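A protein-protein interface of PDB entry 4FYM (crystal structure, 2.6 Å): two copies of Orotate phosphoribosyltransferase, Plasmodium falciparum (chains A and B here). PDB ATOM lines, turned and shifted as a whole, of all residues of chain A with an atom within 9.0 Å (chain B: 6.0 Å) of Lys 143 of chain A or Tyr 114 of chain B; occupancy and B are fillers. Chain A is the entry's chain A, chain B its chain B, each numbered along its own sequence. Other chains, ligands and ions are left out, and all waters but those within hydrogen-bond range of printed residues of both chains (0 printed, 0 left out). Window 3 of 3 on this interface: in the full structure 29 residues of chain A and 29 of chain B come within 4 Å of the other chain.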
ATOM      1  N   GLY A 111       5.795  14.981 -14.299  1.00  0.00           N
ATOM      2  CA  GLY A 111       6.399  13.681 -14.600  1.00  0.00           C
ATOM      3  C   GLY A 111       7.861  13.764 -14.296  1.00  0.00           C
ATOM      4  O   GLY A 111       8.543  14.580 -14.903  1.00  0.00           O
ATOM      5  N   ALA A 112       8.321  12.979 -13.329  1.00  0.00           N
ATOM      6  CA  ALA A 112       9.734  12.944 -12.945  1.00  0.00           C
ATOM      7  C   ALA A 112      10.619  12.529 -14.119  1.00  0.00           C
ATOM      8  O   ALA A 112      10.369  11.520 -14.772  1.00  0.00           O
ATOM      9  CB  ALA A 112       9.930  11.988 -11.795  1.00  0.00           C
ATOM     10  N   SER A 113      11.646  13.305 -14.412  1.00  0.00           N
ATOM     11  CA  SER A 113      12.505  12.971 -15.543  1.00  0.00           C
ATOM     12  C   SER A 113      13.319  11.729 -15.188  1.00  0.00           C
ATOM     13  O   SER A 113      13.721  11.588 -14.026  1.00  0.00           O
ATOM     14  CB  SER A 113      13.449  14.118 -15.850  1.00  0.00           C
ATOM     15  OG  SER A 113      14.239  14.477 -14.698  1.00  0.00           O
ATOM     16  N   TYR A 114      13.551  10.799 -16.113  1.00  0.00           N
ATOM     17  CA  TYR A 114      12.950  10.746 -17.432  1.00  0.00           C
ATOM     18  C   TYR A 114      11.712   9.872 -17.443  1.00  0.00           C
ATOM     19  O   TYR A 114      10.796  10.087 -18.232  1.00  0.00           O
ATOM     20  CB  TYR A 114      13.933  10.134 -18.418  1.00  0.00           C
ATOM     21  CG  TYR A 114      15.013  11.062 -18.912  1.00  0.00           C
ATOM     22  CD1 TYR A 114      14.832  11.801 -20.085  1.00  0.00           C
ATOM     23  CD2 TYR A 114      16.237  11.188 -18.228  1.00  0.00           C
ATOM     24  CE1 TYR A 114      15.793  12.667 -20.542  1.00  0.00           C
ATOM     25  CE2 TYR A 114      17.224  12.041 -18.701  1.00  0.00           C
ATOM     26  CZ  TYR A 114      16.996  12.779 -19.851  1.00  0.00           C
ATOM     27  OH  TYR A 114      17.971  13.652 -20.346  1.00  0.00           O
ATOM     28  N   LYS A 115      11.680   8.896 -16.546  1.00  0.00           N
ATOM     29  CA  LYS A 115      10.703   7.804 -16.627  1.00  0.00           C
ATOM     30  C   LYS A 115       9.272   8.299 -16.568  1.00  0.00           C
ATOM     31  O   LYS A 115       8.391   7.660 -17.129  1.00  0.00           O
ATOM     32  CB  LYS A 115      10.970   6.709 -15.522  1.00  0.00           C
ATOM     33  CG  LYS A 115      12.286   5.958 -15.782  1.00  0.00           C
ATOM     34  CD  LYS A 115      12.909   5.189 -14.607  1.00  0.00           C
ATOM     35  CE  LYS A 115      13.405   6.078 -13.433  1.00  0.00           C
ATOM     36  NZ  LYS A 115      14.882   6.229 -13.439  1.00  0.00           N
ATOM     37  N   ILE A 117       8.056  11.120 -17.595  1.00  0.00           N
ATOM     38  CA  ILE A 117       7.648  12.025 -18.612  1.00  0.00           C
ATOM     39  C   ILE A 117       6.663  11.402 -19.601  1.00  0.00           C
ATOM     40  O   ILE A 117       5.631  11.982 -19.871  1.00  0.00           O
ATOM     41  CB  ILE A 117       8.867  12.666 -19.323  1.00  0.00           C
ATOM     42  CG1 ILE A 117       9.723  13.350 -18.274  1.00  0.00           C
ATOM     43  CG2 ILE A 117       8.428  13.695 -20.344  1.00  0.00           C
ATOM     44  CD1 ILE A 117      10.927  14.087 -18.799  1.00  0.00           C
ATOM     45  N   PRO A 118       6.967  10.234 -20.177  1.00  0.00           N
ATOM     46  CA  PRO A 118       5.934   9.656 -21.060  1.00  0.00           C
ATOM     47  C   PRO A 118       4.713   9.174 -20.310  1.00  0.00           C
ATOM     48  O   PRO A 118       3.606   9.235 -20.868  1.00  0.00           O
ATOM     49  CB  PRO A 118       6.633   8.490 -21.756  1.00  0.00           C
ATOM     50  CG  PRO A 118       7.758   8.142 -20.837  1.00  0.00           C
ATOM     51  CD  PRO A 118       8.141   9.358 -20.049  1.00  0.00           C
ATOM     52  N   TYR A 138       0.438  19.641 -17.525  1.00  0.00           N
ATOM     53  CA  TYR A 138       1.513  18.805 -16.992  1.00  0.00           C
ATOM     54  C   TYR A 138       2.868  19.424 -17.178  1.00  0.00           C
ATOM     55  O   TYR A 138       3.074  20.291 -18.045  1.00  0.00           O
ATOM     56  CB  TYR A 138       1.454  17.402 -17.560  1.00  0.00           C
ATOM     57  CG  TYR A 138       1.316  17.293 -19.059  1.00  0.00           C
ATOM     58  CD1 TYR A 138       2.410  17.294 -19.856  1.00  0.00           C
ATOM     59  CD2 TYR A 138       0.096  17.122 -19.664  1.00  0.00           C
ATOM     60  CE1 TYR A 138       2.317  17.125 -21.220  1.00  0.00           C
ATOM     61  CE2 TYR A 138      -0.016  16.925 -21.045  1.00  0.00           C
ATOM     62  CZ  TYR A 138       1.102  16.916 -21.807  1.00  0.00           C
ATOM     63  OH  TYR A 138       1.030  16.745 -23.194  1.00  0.00           O
ATOM     64  N   TYR A 140       7.345  18.868 -16.546  1.00  0.00           N
ATOM     65  CA  TYR A 140       8.458  17.973 -16.297  1.00  0.00           C
ATOM     66  C   TYR A 140       9.676  18.768 -15.960  1.00  0.00           C
ATOM     67  O   TYR A 140       9.759  19.962 -16.233  1.00  0.00           O
ATOM     68  CB  TYR A 140       8.718  17.043 -17.471  1.00  0.00           C
ATOM     69  CG  TYR A 140       9.065  17.741 -18.758  1.00  0.00           C
ATOM     70  CD1 TYR A 140      10.347  18.216 -18.993  1.00  0.00           C
ATOM     71  CD2 TYR A 140       8.113  17.883 -19.773  1.00  0.00           C
ATOM     72  CE1 TYR A 140      10.677  18.826 -20.191  1.00  0.00           C
ATOM     73  CE2 TYR A 140       8.438  18.490 -20.978  1.00  0.00           C
ATOM     74  CZ  TYR A 140       9.720  18.959 -21.171  1.00  0.00           C
ATOM     75  OH  TYR A 140      10.045  19.541 -22.328  1.00  0.00           O
ATOM     76  N   ASP A 141      10.595  18.125 -15.259  1.00  0.00           N
ATOM     77  CA  ASP A 141      11.868  18.736 -14.884  1.00  0.00           C
ATOM     78  C   ASP A 141      12.955  18.299 -15.831  1.00  0.00           C
ATOM     79  O   ASP A 141      13.017  17.149 -16.185  1.00  0.00           O
ATOM     80  CB  ASP A 141      12.234  18.323 -13.435  1.00  0.00           C
ATOM     81  CG  ASP A 141      12.419  16.812 -13.263  1.00  0.00           C
ATOM     82  OD1 ASP A 141      11.497  16.032 -13.594  1.00  0.00           O
ATOM     83  OD2 ASP A 141      13.460  16.395 -12.717  1.00  0.00           O
ATOM     84  N   ARG A 142      13.879  19.165 -16.136  1.00  0.00           N
ATOM     85  CA  ARG A 142      15.130  18.748 -16.778  1.00  0.00           C
ATOM     86  C   ARG A 142      16.213  18.231 -15.780  1.00  0.00           C
ATOM     87  O   ARG A 142      16.101  18.515 -14.589  1.00  0.00           O
ATOM     88  CB  ARG A 142      15.646  19.896 -17.634  1.00  0.00           C
ATOM     89  CG  ARG A 142      14.639  20.402 -18.645  1.00  0.00           C
ATOM     90  CD  ARG A 142      15.401  21.229 -19.644  1.00  0.00           C
ATOM     91  NE  ARG A 142      14.526  22.085 -20.428  1.00  0.00           N
ATOM     92  CZ  ARG A 142      14.585  23.425 -20.519  1.00  0.00           C
ATOM     93  NH1 ARG A 142      15.545  24.171 -19.927  1.00  0.00           N
ATOM     94  NH2 ARG A 142      13.676  24.051 -21.275  1.00  0.00           N
ATOM     95  N   LYS A 143      17.234  17.516 -16.305  1.00  0.00           N
ATOM     96  CA  LYS A 143      18.256  16.657 -15.640  1.00  0.00           C
ATOM     97  C   LYS A 143      17.664  15.424 -14.866  1.00  0.00           C
ATOM     98  O   LYS A 143      17.782  14.211 -15.210  1.00  0.00           O
ATOM     99  CB  LYS A 143      19.185  17.468 -14.678  1.00  0.00           C
ATOM    100  CG  LYS A 143      19.502  18.942 -14.977  1.00  0.00           C
ATOM    101  CD  LYS A 143      20.990  19.172 -15.183  1.00  0.00           C
ATOM    102  CE  LYS A 143      21.249  20.628 -15.461  1.00  0.00           C
ATOM    103  NZ  LYS A 143      22.638  20.847 -15.932  1.00  0.00           N
ATOM    104  N   ASN A 152      13.938  27.865 -16.055  1.00  0.00           N
ATOM    105  CA  ASN A 152      14.410  26.949 -17.050  1.00  0.00           C
ATOM    106  C   ASN A 152      14.189  25.463 -16.638  1.00  0.00           C
ATOM    107  O   ASN A 152      13.895  24.649 -17.501  1.00  0.00           O
ATOM    108  CB  ASN A 152      15.923  27.173 -17.386  1.00  0.00           C
ATOM    109  CG  ASN A 152      16.195  28.407 -18.269  1.00  0.00           C
ATOM    110  OD1 ASN A 152      15.782  28.448 -19.427  1.00  0.00           O
ATOM    111  ND2 ASN A 152      16.946  29.385 -17.738  1.00  0.00           N
ATOM    112  N   VAL A 153      14.339  25.090 -15.357  1.00  0.00           N
ATOM    113  CA  VAL A 153      14.430  23.657 -15.002  1.00  0.00           C
ATOM    114  C   VAL A 153      13.078  22.949 -15.007  1.00  0.00           C
ATOM    115  O   VAL A 153      13.062  21.740 -15.055  1.00  0.00           O
ATOM    116  CB  VAL A 153      15.218  23.334 -13.651  1.00  0.00           C
ATOM    117  CG1 VAL A 153      16.689  23.588 -13.837  1.00  0.00           C
ATOM    118  CG2 VAL A 153      14.693  24.132 -12.443  1.00  0.00           C
ATOM    119  N   ILE A 154      11.986  23.679 -14.809  1.00  0.00           N
ATOM    120  CA  ILE A 154      10.622  23.134 -14.868  1.00  0.00           C
ATOM    121  C   ILE A 154       9.912  23.665 -16.125  1.00  0.00           C
ATOM    122  O   ILE A 154       9.858  24.837 -16.362  1.00  0.00           O
ATOM    123  CB  ILE A 154       9.795  23.480 -13.612  1.00  0.00           C
ATOM    124  CG1 ILE A 154      10.512  23.098 -12.297  1.00  0.00           C
ATOM    125  CG2 ILE A 154       8.484  22.761 -13.634  1.00  0.00           C
ATOM    126  CD1 ILE A 154      10.861  21.622 -12.114  1.00  0.00           C
ATOM    127  N   VAL A 155       9.398  22.763 -16.938  1.00  0.00           N
ATOM    128  CA  VAL A 155       8.835  23.096 -18.230  1.00  0.00           C
ATOM    129  C   VAL A 155       7.354  22.831 -18.186  1.00  0.00           C
ATOM    130  O   VAL A 155       6.907  21.803 -17.662  1.00  0.00           O
ATOM    131  CB  VAL A 155       9.452  22.225 -19.322  1.00  0.00           C
ATOM    132  CG1 VAL A 155       8.872  22.547 -20.689  1.00  0.00           C
ATOM    133  CG2 VAL A 155      10.946  22.423 -19.341  1.00  0.00           C
ATOM    134  N   GLU A 198      15.168  15.227  -4.888  1.00  0.00           N
ATOM    135  CA  GLU A 198      15.911  16.044  -5.828  1.00  0.00           C
ATOM    136  C   GLU A 198      14.937  16.962  -6.623  1.00  0.00           C
ATOM    137  O   GLU A 198      15.190  18.187  -6.808  1.00  0.00           O
ATOM    138  CB  GLU A 198      16.734  15.091  -6.722  1.00  0.00           C
ATOM    139  CG  GLU A 198      17.669  15.767  -7.704  1.00  0.00           C
ATOM    140  CD  GLU A 198      18.422  14.775  -8.578  1.00  0.00           C
ATOM    141  OE1 GLU A 198      18.493  13.577  -8.200  1.00  0.00           O
ATOM    142  OE2 GLU A 198      18.954  15.218  -9.628  1.00  0.00           O
ATOM    143  N   ILE A 199      13.779  16.422  -6.977  1.00  0.00           N
ATOM    144  CA  ILE A 199      12.769  17.233  -7.624  1.00  0.00           C
ATOM    145  C   ILE A 199      12.249  18.304  -6.666  1.00  0.00           C
ATOM    146  O   ILE A 199      12.028  19.470  -7.093  1.00  0.00           O
ATOM    147  CB  ILE A 199      11.625  16.387  -8.214  1.00  0.00           C
ATOM    148  CG1 ILE A 199      12.181  15.489  -9.320  1.00  0.00           C
ATOM    149  CG2 ILE A 199      10.561  17.267  -8.823  1.00  0.00           C
ATOM    150  CD1 ILE A 199      11.212  14.420  -9.807  1.00  0.00           C
ATOM    151  N   LYS A 202      14.539  21.211  -6.697  1.00  0.00           N
ATOM    152  CA  LYS A 202      14.330  22.058  -7.874  1.00  0.00           C
ATOM    153  C   LYS A 202      13.120  22.935  -7.726  1.00  0.00           C
ATOM    154  O   LYS A 202      13.115  24.073  -8.224  1.00  0.00           O
ATOM    155  CB  LYS A 202      14.218  21.230  -9.161  1.00  0.00           C
ATOM    156  CG  LYS A 202      15.479  20.434  -9.483  1.00  0.00           C
ATOM    157  CD  LYS A 202      15.233  19.449 -10.597  1.00  0.00           C
ATOM    158  CE  LYS A 202      16.516  18.777 -11.030  1.00  0.00           C
ATOM    159  NZ  LYS A 202      16.166  17.546 -11.786  1.00  0.00           N
ATOM    160  N   ALA B 112      12.094  12.732 -29.324  1.00  0.00           N
ATOM    161  CA  ALA B 112      13.345  13.533 -29.090  1.00  0.00           C
ATOM    162  C   ALA B 112      13.336  14.203 -27.718  1.00  0.00           C
ATOM    163  O   ALA B 112      12.354  14.856 -27.342  1.00  0.00           O
ATOM    164  CB  ALA B 112      13.486  14.592 -30.166  1.00  0.00           C
ATOM    165  N   SER B 113      14.396  14.044 -26.965  1.00  0.00           N
ATOM    166  CA  SER B 113      14.408  14.618 -25.618  1.00  0.00           C
ATOM    167  C   SER B 113      14.536  16.146 -25.749  1.00  0.00           C
ATOM    168  O   SER B 113      15.248  16.586 -26.643  1.00  0.00           O
ATOM    169  CB  SER B 113      15.583  14.057 -24.812  1.00  0.00           C
ATOM    170  OG  SER B 113      16.832  14.277 -25.496  1.00  0.00           O
ATOM    171  N   TYR B 114      13.863  16.955 -24.932  1.00  0.00           N
ATOM    172  CA  TYR B 114      12.852  16.531 -23.994  1.00  0.00           C
ATOM    173  C   TYR B 114      11.463  16.634 -24.599  1.00  0.00           C
ATOM    174  O   TYR B 114      10.537  15.907 -24.204  1.00  0.00           O
ATOM    175  CB  TYR B 114      12.884  17.432 -22.772  1.00  0.00           C
ATOM    176  CG  TYR B 114      13.982  17.175 -21.773  1.00  0.00           C
ATOM    177  CD1 TYR B 114      13.779  16.309 -20.699  1.00  0.00           C
ATOM    178  CD2 TYR B 114      15.226  17.769 -21.907  1.00  0.00           C
ATOM    179  CE1 TYR B 114      14.787  16.035 -19.802  1.00  0.00           C
ATOM    180  CE2 TYR B 114      16.247  17.503 -21.002  1.00  0.00           C
ATOM    181  CZ  TYR B 114      16.015  16.648 -19.955  1.00  0.00           C
ATOM    182  OH  TYR B 114      17.026  16.383 -19.051  1.00  0.00           O
ATOM    183  N   LYS B 115      11.307  17.546 -25.559  1.00  0.00           N
ATOM    184  CA  LYS B 115       9.970  17.988 -25.997  1.00  0.00           C
ATOM    185  C   LYS B 115       9.154  16.896 -26.617  1.00  0.00           C
ATOM    186  O   LYS B 115       7.932  16.896 -26.486  1.00  0.00           O
ATOM    187  CB  LYS B 115      10.074  19.166 -26.979  1.00  0.00           C
ATOM    188  CG  LYS B 115      10.600  20.397 -26.305  1.00  0.00           C
ATOM    189  CD  LYS B 115      11.485  21.106 -27.301  1.00  0.00           C
ATOM    190  CE  LYS B 115      12.397  22.080 -26.630  1.00  0.00           C
ATOM    191  NZ  LYS B 115      13.425  22.661 -27.515  1.00  0.00           N
ATOM    192  N   GLY B 116       9.835  16.005 -27.342  1.00  0.00           N
ATOM    193  CA  GLY B 116       9.187  14.862 -27.968  1.00  0.00           C
ATOM    194  C   GLY B 116       8.700  13.791 -27.000  1.00  0.00           C
ATOM    195  O   GLY B 116       7.906  12.959 -27.383  1.00  0.00           O
ATOM    196  N   ILE B 117       9.186  13.776 -25.770  1.00  0.00           N
ATOM    197  CA  ILE B 117       8.948  12.653 -24.928  1.00  0.00           C
ATOM    198  C   ILE B 117       7.478  12.546 -24.516  1.00  0.00           C
ATOM    199  O   ILE B 117       6.893  11.494 -24.636  1.00  0.00           O
ATOM    200  CB  ILE B 117       9.914  12.609 -23.740  1.00  0.00           C
ATOM    201  CG1 ILE B 117      11.349  12.579 -24.272  1.00  0.00           C
ATOM    202  CG2 ILE B 117       9.676  11.366 -22.863  1.00  0.00           C
ATOM    203  CD1 ILE B 117      12.434  12.487 -23.207  1.00  0.00           C
ATOM    204  N   PRO B 118       6.874  13.610 -24.022  1.00  0.00           N
ATOM    205  CA  PRO B 118       5.443  13.485 -23.705  1.00  0.00           C
ATOM    206  C   PRO B 118       4.583  13.361 -24.922  1.00  0.00           C
ATOM    207  O   PRO B 118       3.534  12.684 -24.870  1.00  0.00           O
ATOM    208  CB  PRO B 118       5.113  14.757 -22.941  1.00  0.00           C
ATOM    209  CG  PRO B 118       6.153  15.736 -23.361  1.00  0.00           C
ATOM    210  CD  PRO B 118       7.384  14.968 -23.766  1.00  0.00           C
ATOM    211  N   ARG B 142      18.304   9.866 -23.736  1.00  0.00           N
ATOM    212  CA  ARG B 142      18.771  10.722 -22.665  1.00  0.00           C
ATOM    213  C   ARG B 142      19.746  11.859 -23.213  1.00  0.00           C
ATOM    214  O   ARG B 142      20.295  11.721 -24.348  1.00  0.00           O
ATOM    215  CB  ARG B 142      19.389   9.871 -21.543  1.00  0.00           C
ATOM    216  CG  ARG B 142      18.424   8.805 -20.971  1.00  0.00           C
ATOM    217  CD  ARG B 142      18.723   7.795 -19.749  1.00  0.00           C
ATOM    218  NE  ARG B 142      18.788   8.280 -18.333  1.00  0.00           N
ATOM    219  CZ  ARG B 142      17.870   8.108 -17.329  1.00  0.00           C
ATOM    220  NH1 ARG B 142      16.685   7.500 -17.514  1.00  0.00           N
ATOM    221  NH2 ARG B 142      18.125   8.599 -16.097  1.00  0.00           N
ATOM    222  N   LYS B 143      19.954  12.913 -22.388  1.00  0.00           N
ATOM    223  CA  LYS B 143      20.659  14.213 -22.627  1.00  0.00           C
ATOM    224  C   LYS B 143      20.176  15.192 -23.754  1.00  0.00           C
ATOM    225  O   LYS B 143      19.277  16.057 -23.576  1.00  0.00           O
ATOM    226  CB  LYS B 143      22.182  13.950 -22.693  1.00  0.00           C
ATOM    227  CG  LYS B 143      22.711  13.292 -21.423  1.00  0.00           C
ATOM    228  CD  LYS B 143      24.167  13.618 -21.213  1.00  0.00           C
ATOM    229  CE  LYS B 143      24.714  12.804 -20.068  1.00  0.00           C
ATOM    230  NZ  LYS B 143      26.066  13.279 -19.674  1.00  0.00           N
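OH of Tyr 114 of chain B sits at hydrogen-bond distance from OH of Tyr 114 of chain A, 3.2 Å away. N of Lys 143 of chain A lies within hydrogen-bond range of OH of Tyr 114 of chain B, at 3.0 Å. The side-chain hydroxyl (OH) of Tyr 114 of chain A sits at hydrogen-bond distance from the backbone NH (N) of Lys 143 of chain B.
The backbone carbonyl oxygen (O) of Val 153 of chain A lies within hydrogen-bond range of the backbone NH (N) of Arg 142 of chain A (2.9 Å). The backbone carbonyl oxygen (O) of Arg 142 of chain A sits at hydrogen-bond distance from the side-chain amino group (NZ) of Lys 202 of chain A (3.0 Å). NH1 of Arg 142 of chain A is in hydrogen-bond range of O of Asn 152 of chain A (3.0 Å). The backbone carbonyl oxygen of Tyr 140 of chain A is in hydrogen-bond range of the backbone NH of Val 155 of chain A (2.9 Å).
Tyr 114 of chain A touches Ile 117 of chain B. Arg 142 of chain B touches Tyr 114 of chain A (CZ to CD2, 3.6 Å). CG2 of Ile 117 of chain A touches CG2 of Ile 117 of chain B, at 3.7 Å. Ile 117 of chain A touches Pro 118 of chain B. Pro 118 of chain A touches Ile 117 of chain B. CB of Tyr 114 of chain B touches OH of Tyr 140 of chain A (3.6 Å). Lys 115 of chain B touches Tyr 140 of chain A (CA to OH, 3.98 Å). Arg 142 of chain A touches Tyr 114 of chain B (CA to OH, 3.8 Å).
Of the printed residues of chain B, Ile 117 of chain A touches Ile 117 and Pro 118. Of the printed residues of chain B, Tyr 140 of chain A touches Tyr 114 and Lys 115. Printed residues of chain B within 4 Å of Lys 143 of chain A: Tyr 114 (3.0 Å). Of chain A, only Tyr 114 (3.2 Å), Tyr 140 (3.6 Å), Arg 142 (3.8 Å) and Lys 143 (3.0 Å) come within 4 Å of Tyr 114 of chain B. The nearest residue of chain B that does not touch Lys 143 of chain A is Arg 142 of chain B (5.7 Å). The nearest residue of chain A that does not touch Tyr 114 of chain B is Ile 117 of chain A (4.1 Å). The nearest printed residue of chain B that does not touch Ile 117 of chain A is Tyr 114 of chain B (4.1 Å).
Hydrophobic or aromatic side chains of chain B that line the printed part of chain A: Tyr 114, Ile 117 and Pro 118. Of the 19 printed residues of chain A, 6 touch a printed residue of chain B. Among the printed residues, 11 pairs touch across the chains. Among the printed residues, no Asp or Glu carboxylate lies within 4 Å of a Lys or Arg side-chain nitrogen of the other chain.
Tyr 114 of chain A touches its own counterpart, Tyr 114 of chain B. Tyr 114 of chain A touches Ile 117 of chain B, but with the chains exchanged Ile 117 of chain A does not touch Tyr 114 of chain B (4.1 Å). Ile 117 of chain B touches its own counterpart, Ile 117 of chain A. Ile 117 of chain A touches Pro 118 of chain B, and with the chains exchanged Pro 118 of chain A touches Ile 117 of chain B. Of the 11 pairs that touch across the chains among the printed residues, 8 have their exchanged pair printed and touching as well.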
